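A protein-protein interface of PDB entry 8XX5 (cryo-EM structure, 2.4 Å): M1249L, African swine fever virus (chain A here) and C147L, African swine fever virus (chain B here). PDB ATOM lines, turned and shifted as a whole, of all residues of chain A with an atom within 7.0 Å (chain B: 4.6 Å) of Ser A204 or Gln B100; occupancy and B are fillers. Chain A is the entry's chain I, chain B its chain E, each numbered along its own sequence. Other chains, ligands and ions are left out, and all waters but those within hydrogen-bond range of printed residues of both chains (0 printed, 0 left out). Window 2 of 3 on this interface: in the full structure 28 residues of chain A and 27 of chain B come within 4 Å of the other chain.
Thr A201 touches none of the printed residues of chain B.
Printed residues of chain B within 4 Å of Tyr A203: Asp B139.
Ser A204 touches just these residues of chain B: Gln B100 (3.1 Å), Phe B103 (3.1 Å) and Asn B104 (3.4 Å).
Of the printed residues of chain B, Ser A206 touches Phe B103 (3.9 Å) and Asn B104 (3.1 Å).
Ile B97 touches none of the printed residues of chain A.
Gln B100 touches just one residue of chain A: Ser A204 (3.1 Å).
Of the printed residues of chain A, Asp B139 touches Tyr A203 and Arg A222.
The nearest residue of chain A that does not touch Gln B100 is Arg A222 (5.5 Å).
Hydrophobic or aromatic side chains of chain B that line the printed part of chain A: Phe B103.
CB of Ser A204 touches ND2 of Asn B104, 3.4 Å away.
Phe B103 touches Ser A206.
Phe B103 touches Arg A222.
The chain-end carboxylate (OXT) of Asp B139 lies close to the side-chain hydroxyl (OH) of Tyr A203, 3.3 Å away.
OG of Ser A204 is in hydrogen-bond range of OE1 of Gln B100 (3.1 Å).
O of Asn B104 lies within hydrogen-bond range of OG of Ser A206 (3.1 Å).
The guanidinium group (NH2) of Arg A222 lies within salt-bridge range of the side-chain carboxylate (OD2) of Asp B139, at 2.4 Å.
O of Phe B103 lies close to O of Ser A204, 3.1 Å away.
The backbone carbonyl oxygen (O) of Ser A204 is in hydrogen-bond range of the guanidinium group (NH1) of Arg A222 (2.6 Å).
The side-chain amide oxygen (OE1) of Gln B100 sits at hydrogen-bond distance from the side-chain hydroxyl (OH) of Tyr B91, 3.5 Å away.
O of Gln B100 sits at hydrogen-bond distance from ND2 of Asn B104 (2.7 Å).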
ATOM      1  N   LEU A 199      26.218  25.707 -26.927  1.00  0.00           N
ATOM      2  CA  LEU A 199      26.172  25.392 -25.508  1.00  0.00           C
ATOM      3  C   LEU A 199      25.265  24.205 -25.201  1.00  0.00           C
ATOM      4  O   LEU A 199      25.442  23.562 -24.161  1.00  0.00           O
ATOM      5  CB  LEU A 199      25.718  26.619 -24.712  1.00  0.00           C
ATOM      6  CG  LEU A 199      25.930  26.550 -23.199  1.00  0.00           C
ATOM      7  CD1 LEU A 199      27.411  26.469 -22.883  1.00  0.00           C
ATOM      8  CD2 LEU A 199      25.301  27.739 -22.500  1.00  0.00           C
ATOM      9  N   SER A 200      24.312  23.893 -26.084  1.00  0.00           N
ATOM     10  CA  SER A 200      23.432  22.752 -25.852  1.00  0.00           C
ATOM     11  C   SER A 200      24.200  21.437 -25.869  1.00  0.00           C
ATOM     12  O   SER A 200      23.880  20.524 -25.099  1.00  0.00           O
ATOM     13  CB  SER A 200      22.316  22.722 -26.893  1.00  0.00           C
ATOM     14  OG  SER A 200      22.797  23.117 -28.164  1.00  0.00           O
ATOM     15  N   THR A 201      25.210  21.320 -26.733  1.00  0.00           N
ATOM     16  CA  THR A 201      26.041  20.124 -26.779  1.00  0.00           C
ATOM     17  C   THR A 201      26.891  19.956 -25.529  1.00  0.00           C
ATOM     18  O   THR A 201      27.488  18.891 -25.342  1.00  0.00           O
ATOM     19  CB  THR A 201      26.951  20.163 -28.008  1.00  0.00           C
ATOM     20  OG1 THR A 201      28.099  20.973 -27.726  1.00  0.00           O
ATOM     21  CG2 THR A 201      26.211  20.744 -29.202  1.00  0.00           C
ATOM     22  N   MET A 202      26.959  20.976 -24.677  1.00  0.00           N
ATOM     23  CA  MET A 202      27.827  20.968 -23.514  1.00  0.00           C
ATOM     24  C   MET A 202      27.139  21.395 -22.228  1.00  0.00           C
ATOM     25  O   MET A 202      27.784  21.384 -21.174  1.00  0.00           O
ATOM     26  CB  MET A 202      29.033  21.881 -23.762  1.00  0.00           C
ATOM     27  CG  MET A 202      28.666  23.088 -24.602  1.00  0.00           C
ATOM     28  SD  MET A 202      30.090  23.964 -25.245  1.00  0.00           S
ATOM     29  CE  MET A 202      31.145  23.841 -23.819  1.00  0.00           C
ATOM     30  N   TYR A 203      25.869  21.782 -22.277  1.00  0.00           N
ATOM     31  CA  TYR A 203      25.134  22.152 -21.078  1.00  0.00           C
ATOM     32  C   TYR A 203      23.654  21.957 -21.365  1.00  0.00           C
ATOM     33  O   TYR A 203      23.222  22.028 -22.518  1.00  0.00           O
ATOM     34  CB  TYR A 203      25.437  23.596 -20.663  1.00  0.00           C
ATOM     35  CG  TYR A 203      24.959  23.965 -19.278  1.00  0.00           C
ATOM     36  CD1 TYR A 203      25.662  23.566 -18.151  1.00  0.00           C
ATOM     37  CD2 TYR A 203      23.810  24.716 -19.097  1.00  0.00           C
ATOM     38  CE1 TYR A 203      25.228  23.903 -16.884  1.00  0.00           C
ATOM     39  CE2 TYR A 203      23.368  25.055 -17.836  1.00  0.00           C
ATOM     40  CZ  TYR A 203      24.082  24.650 -16.734  1.00  0.00           C
ATOM     41  OH  TYR A 203      23.645  24.991 -15.476  1.00  0.00           O
ATOM     42  N   SER A 204      22.882  21.712 -20.307  1.00  0.00           N
ATOM     43  CA  SER A 204      21.468  21.360 -20.443  1.00  0.00           C
ATOM     44  C   SER A 204      20.617  22.599 -20.733  1.00  0.00           C
ATOM     45  O   SER A 204      19.719  22.974 -19.981  1.00  0.00           O
ATOM     46  CB  SER A 204      20.993  20.639 -19.190  1.00  0.00           C
ATOM     47  OG  SER A 204      21.335  21.368 -18.025  1.00  0.00           O
ATOM     48  N   VAL A 205      20.924  23.242 -21.857  1.00  0.00           N
ATOM     49  CA  VAL A 205      20.226  24.449 -22.288  1.00  0.00           C
ATOM     50  C   VAL A 205      19.671  24.292 -23.696  1.00  0.00           C
ATOM     51  O   VAL A 205      19.707  25.245 -24.482  1.00  0.00           O
ATOM     52  CB  VAL A 205      21.136  25.687 -22.207  1.00  0.00           C
ATOM     53  CG1 VAL A 205      21.269  26.147 -20.771  1.00  0.00           C
ATOM     54  CG2 VAL A 205      22.500  25.371 -22.798  1.00  0.00           C
ATOM     55  N   SER A 206      19.198  23.087 -24.037  1.00  0.00           N
ATOM     56  CA  SER A 206      18.628  22.806 -25.351  1.00  0.00           C
ATOM     57  C   SER A 206      17.698  23.933 -25.784  1.00  0.00           C
ATOM     58  O   SER A 206      16.637  24.134 -25.182  1.00  0.00           O
ATOM     59  CB  SER A 206      17.874  21.477 -25.339  1.00  0.00           C
ATOM     60  OG  SER A 206      16.740  21.528 -26.189  1.00  0.00           O
ATOM     61  N   PRO A 207      18.066  24.685 -26.816  1.00  0.00           N
ATOM     62  CA  PRO A 207      17.375  25.946 -27.097  1.00  0.00           C
ATOM     63  C   PRO A 207      16.095  25.768 -27.893  1.00  0.00           C
ATOM     64  O   PRO A 207      15.980  24.906 -28.767  1.00  0.00           O
ATOM     65  CB  PRO A 207      18.409  26.736 -27.914  1.00  0.00           C
ATOM     66  CG  PRO A 207      19.704  25.966 -27.785  1.00  0.00           C
ATOM     67  CD  PRO A 207      19.286  24.549 -27.623  1.00  0.00           C
ATOM     68  N   ASP A 219      16.932  30.448 -19.756  1.00  0.00           N
ATOM     69  CA  ASP A 219      18.071  29.545 -19.854  1.00  0.00           C
ATOM     70  C   ASP A 219      19.401  30.276 -19.751  1.00  0.00           C
ATOM     71  O   ASP A 219      20.364  29.711 -19.224  1.00  0.00           O
ATOM     72  CB  ASP A 219      18.012  28.763 -21.168  1.00  0.00           C
ATOM     73  CG  ASP A 219      16.819  27.831 -21.237  1.00  0.00           C
ATOM     74  OD1 ASP A 219      16.102  27.704 -20.221  1.00  0.00           O
ATOM     75  OD2 ASP A 219      16.600  27.224 -22.306  1.00  0.00           O
ATOM     76  N   ARG A 222      19.866  30.727 -15.673  1.00  0.00           N
ATOM     77  CA  ARG A 222      20.259  29.616 -14.812  1.00  0.00           C
ATOM     78  C   ARG A 222      21.738  29.289 -14.963  1.00  0.00           C
ATOM     79  O   ARG A 222      22.427  29.023 -13.972  1.00  0.00           O
ATOM     80  CB  ARG A 222      19.414  28.386 -15.128  1.00  0.00           C
ATOM     81  CG  ARG A 222      18.992  28.304 -16.575  1.00  0.00           C
ATOM     82  CD  ARG A 222      18.289  26.998 -16.880  1.00  0.00           C
ATOM     83  NE  ARG A 222      19.174  25.862 -16.659  1.00  0.00           N
ATOM     84  CZ  ARG A 222      19.250  24.809 -17.459  1.00  0.00           C
ATOM     85  NH1 ARG A 222      18.515  24.721 -18.555  1.00  0.00           N
ATOM     86  NH2 ARG A 222      20.094  23.826 -17.160  1.00  0.00           N
ATOM     87  N   GLU A 245      32.193  21.182 -17.918  1.00  0.00           N
ATOM     88  CA  GLU A 245      31.712  19.867 -18.331  1.00  0.00           C
ATOM     89  C   GLU A 245      32.797  18.811 -18.183  1.00  0.00           C
ATOM     90  O   GLU A 245      32.528  17.700 -17.709  1.00  0.00           O
ATOM     91  CB  GLU A 245      31.200  19.896 -19.771  1.00  0.00           C
ATOM     92  CG  GLU A 245      31.137  18.503 -20.394  1.00  0.00           C
ATOM     93  CD  GLU A 245      30.144  18.391 -21.528  1.00  0.00           C
ATOM     94  OE1 GLU A 245      29.085  19.037 -21.447  1.00  0.00           O
ATOM     95  OE2 GLU A 245      30.422  17.659 -22.499  1.00  0.00           O
ATOM     96  N   LEU B  87      17.652  10.820 -22.378  1.00  0.00           N
ATOM     97  CA  LEU B  87      18.789  11.662 -22.042  1.00  0.00           C
ATOM     98  C   LEU B  87      20.077  11.095 -22.626  1.00  0.00           C
ATOM     99  O   LEU B  87      20.241   9.881 -22.774  1.00  0.00           O
ATOM    100  CB  LEU B  87      18.927  11.794 -20.527  1.00  0.00           C
ATOM    101  CG  LEU B  87      18.289  13.011 -19.859  1.00  0.00           C
ATOM    102  CD1 LEU B  87      18.717  13.074 -18.407  1.00  0.00           C
ATOM    103  CD2 LEU B  87      18.660  14.290 -20.588  1.00  0.00           C
ATOM    104  N   TYR B  91      22.958   9.827 -15.579  1.00  0.00           N
ATOM    105  CA  TYR B  91      22.903  10.292 -14.204  1.00  0.00           C
ATOM    106  C   TYR B  91      22.406   9.160 -13.317  1.00  0.00           C
ATOM    107  O   TYR B  91      21.583   8.340 -13.733  1.00  0.00           O
ATOM    108  CB  TYR B  91      21.996  11.519 -14.062  1.00  0.00           C
ATOM    109  CG  TYR B  91      22.324  12.626 -15.038  1.00  0.00           C
ATOM    110  CD1 TYR B  91      21.749  12.658 -16.300  1.00  0.00           C
ATOM    111  CD2 TYR B  91      23.217  13.632 -14.700  1.00  0.00           C
ATOM    112  CE1 TYR B  91      22.050  13.661 -17.194  1.00  0.00           C
ATOM    113  CE2 TYR B  91      23.524  14.640 -15.589  1.00  0.00           C
ATOM    114  CZ  TYR B  91      22.939  14.648 -16.835  1.00  0.00           C
ATOM    115  OH  TYR B  91      23.238  15.652 -17.727  1.00  0.00           O
ATOM    116  N   ASP B  96      17.958  13.783 -10.758  1.00  0.00           N
ATOM    117  CA  ASP B  96      18.850  14.456 -11.695  1.00  0.00           C
ATOM    118  C   ASP B  96      18.426  14.203 -13.134  1.00  0.00           C
ATOM    119  O   ASP B  96      18.484  15.108 -13.972  1.00  0.00           O
ATOM    120  CB  ASP B  96      20.291  13.999 -11.473  1.00  0.00           C
ATOM    121  CG  ASP B  96      20.805  14.350 -10.095  1.00  0.00           C
ATOM    122  OD1 ASP B  96      20.603  15.503  -9.658  1.00  0.00           O
ATOM    123  OD2 ASP B  96      21.409  13.472  -9.445  1.00  0.00           O
ATOM    124  N   ILE B  97      17.997  12.978 -13.437  1.00  0.00           N
ATOM    125  CA  ILE B  97      17.557  12.660 -14.792  1.00  0.00           C
ATOM    126  C   ILE B  97      16.345  13.502 -15.168  1.00  0.00           C
ATOM    127  O   ILE B  97      16.275  14.060 -16.267  1.00  0.00           O
ATOM    128  CB  ILE B  97      17.260  11.156 -14.922  1.00  0.00           C
ATOM    129  CG1 ILE B  97      18.536  10.339 -14.738  1.00  0.00           C
ATOM    130  CG2 ILE B  97      16.644  10.855 -16.269  1.00  0.00           C
ATOM    131  CD1 ILE B  97      18.280   8.894 -14.402  1.00  0.00           C
ATOM    132  N   ALA B  98      15.374  13.610 -14.259  1.00  0.00           N
ATOM    133  CA  ALA B  98      14.184  14.410 -14.535  1.00  0.00           C
ATOM    134  C   ALA B  98      14.526  15.889 -14.674  1.00  0.00           C
ATOM    135  O   ALA B  98      13.982  16.579 -15.547  1.00  0.00           O
ATOM    136  CB  ALA B  98      13.145  14.198 -13.436  1.00  0.00           C
ATOM    137  N   LYS B  99      15.423  16.393 -13.823  1.00  0.00           N
ATOM    138  CA  LYS B  99      15.831  17.790 -13.921  1.00  0.00           C
ATOM    139  C   LYS B  99      16.512  18.075 -15.253  1.00  0.00           C
ATOM    140  O   LYS B  99      16.241  19.098 -15.890  1.00  0.00           O
ATOM    141  CB  LYS B  99      16.757  18.148 -12.760  1.00  0.00           C
ATOM    142  CG  LYS B  99      16.077  18.909 -11.636  1.00  0.00           C
ATOM    143  CD  LYS B  99      16.770  18.683 -10.301  1.00  0.00           C
ATOM    144  CE  LYS B  99      18.260  18.431 -10.468  1.00  0.00           C
ATOM    145  NZ  LYS B  99      19.052  19.098  -9.403  1.00  0.00           N
ATOM    146  N   GLN B 100      17.394  17.176 -15.695  1.00  0.00           N
ATOM    147  CA  GLN B 100      18.056  17.368 -16.981  1.00  0.00           C
ATOM    148  C   GLN B 100      17.085  17.207 -18.143  1.00  0.00           C
ATOM    149  O   GLN B 100      17.236  17.878 -19.168  1.00  0.00           O
ATOM    150  CB  GLN B 100      19.225  16.395 -17.122  1.00  0.00           C
ATOM    151  CG  GLN B 100      20.278  16.525 -16.036  1.00  0.00           C
ATOM    152  CD  GLN B 100      20.823  17.931 -15.908  1.00  0.00           C
ATOM    153  OE1 GLN B 100      21.390  18.476 -16.852  1.00  0.00           O
ATOM    154  NE2 GLN B 100      20.658  18.525 -14.733  1.00  0.00           N
ATOM    155  N   GLU B 101      16.091  16.325 -18.008  1.00  0.00           N
ATOM    156  CA  GLU B 101      15.059  16.207 -19.033  1.00  0.00           C
ATOM    157  C   GLU B 101      14.282  17.505 -19.174  1.00  0.00           C
ATOM    158  O   GLU B 101      13.976  17.936 -20.291  1.00  0.00           O
ATOM    159  CB  GLU B 101      14.106  15.061 -18.698  1.00  0.00           C
ATOM    160  CG  GLU B 101      14.653  13.675 -18.955  1.00  0.00           C
ATOM    161  CD  GLU B 101      13.574  12.614 -18.897  1.00  0.00           C
ATOM    162  OE1 GLU B 101      12.395  12.952 -19.127  1.00  0.00           O
ATOM    163  OE2 GLU B 101      13.902  11.444 -18.616  1.00  0.00           O
ATOM    164  N   LEU B 102      13.937  18.131 -18.049  1.00  0.00           N
ATOM    165  CA  LEU B 102      13.274  19.429 -18.111  1.00  0.00           C
ATOM    166  C   LEU B 102      14.196  20.491 -18.700  1.00  0.00           C
ATOM    167  O   LEU B 102      13.758  21.327 -19.499  1.00  0.00           O
ATOM    168  CB  LEU B 102      12.790  19.845 -16.723  1.00  0.00           C
ATOM    169  CG  LEU B 102      12.038  21.177 -16.668  1.00  0.00           C
ATOM    170  CD1 LEU B 102      10.776  21.115 -17.511  1.00  0.00           C
ATOM    171  CD2 LEU B 102      11.705  21.551 -15.239  1.00  0.00           C
ATOM    172  N   PHE B 103      15.476  20.474 -18.320  1.00  0.00           N
ATOM    173  CA  PHE B 103      16.414  21.472 -18.824  1.00  0.00           C
ATOM    174  C   PHE B 103      16.740  21.243 -20.295  1.00  0.00           C
ATOM    175  O   PHE B 103      16.923  22.203 -21.051  1.00  0.00           O
ATOM    176  CB  PHE B 103      17.690  21.467 -17.987  1.00  0.00           C
ATOM    177  CG  PHE B 103      17.504  21.994 -16.597  1.00  0.00           C
ATOM    178  CD1 PHE B 103      16.560  22.974 -16.336  1.00  0.00           C
ATOM    179  CD2 PHE B 103      18.275  21.518 -15.553  1.00  0.00           C
ATOM    180  CE1 PHE B 103      16.388  23.462 -15.060  1.00  0.00           C
ATOM    181  CE2 PHE B 103      18.105  22.003 -14.274  1.00  0.00           C
ATOM    182  CZ  PHE B 103      17.162  22.977 -14.028  1.00  0.00           C
ATOM    183  N   ASN B 104      16.818  19.984 -20.719  1.00  0.00           N
ATOM    184  CA  ASN B 104      17.089  19.657 -22.113  1.00  0.00           C
ATOM    185  C   ASN B 104      15.832  19.636 -22.966  1.00  0.00           C
ATOM    186  O   ASN B 104      15.910  19.281 -24.146  1.00  0.00           O
ATOM    187  CB  ASN B 104      17.805  18.308 -22.215  1.00  0.00           C
ATOM    188  CG  ASN B 104      19.256  18.386 -21.786  1.00  0.00           C
ATOM    189  OD1 ASN B 104      20.113  18.832 -22.545  1.00  0.00           O
ATOM    190  ND2 ASN B 104      19.537  17.952 -20.565  1.00  0.00           N
ATOM    191  N   ASP B 139      20.339  25.179 -11.362  1.00  0.00           N
ATOM    192  CA  ASP B 139      21.215  24.064 -11.703  1.00  0.00           C
ATOM    193  C   ASP B 139      22.672  24.427 -11.441  1.00  0.00           C
ATOM    194  O   ASP B 139      23.019  24.917 -10.366  1.00  0.00           O
ATOM    195  CB  ASP B 139      21.032  23.660 -13.166  1.00  0.00           C
ATOM    196  CG  ASP B 139      20.920  24.853 -14.086  1.00  0.00           C
ATOM    197  OD1 ASP B 139      20.424  25.903 -13.631  1.00  0.00           O
ATOM    198  OD2 ASP B 139      21.331  24.744 -15.260  1.00  0.00           O
ATOM    199  OXT ASP B 139      23.535  24.238 -12.297  1.00  0.00           O
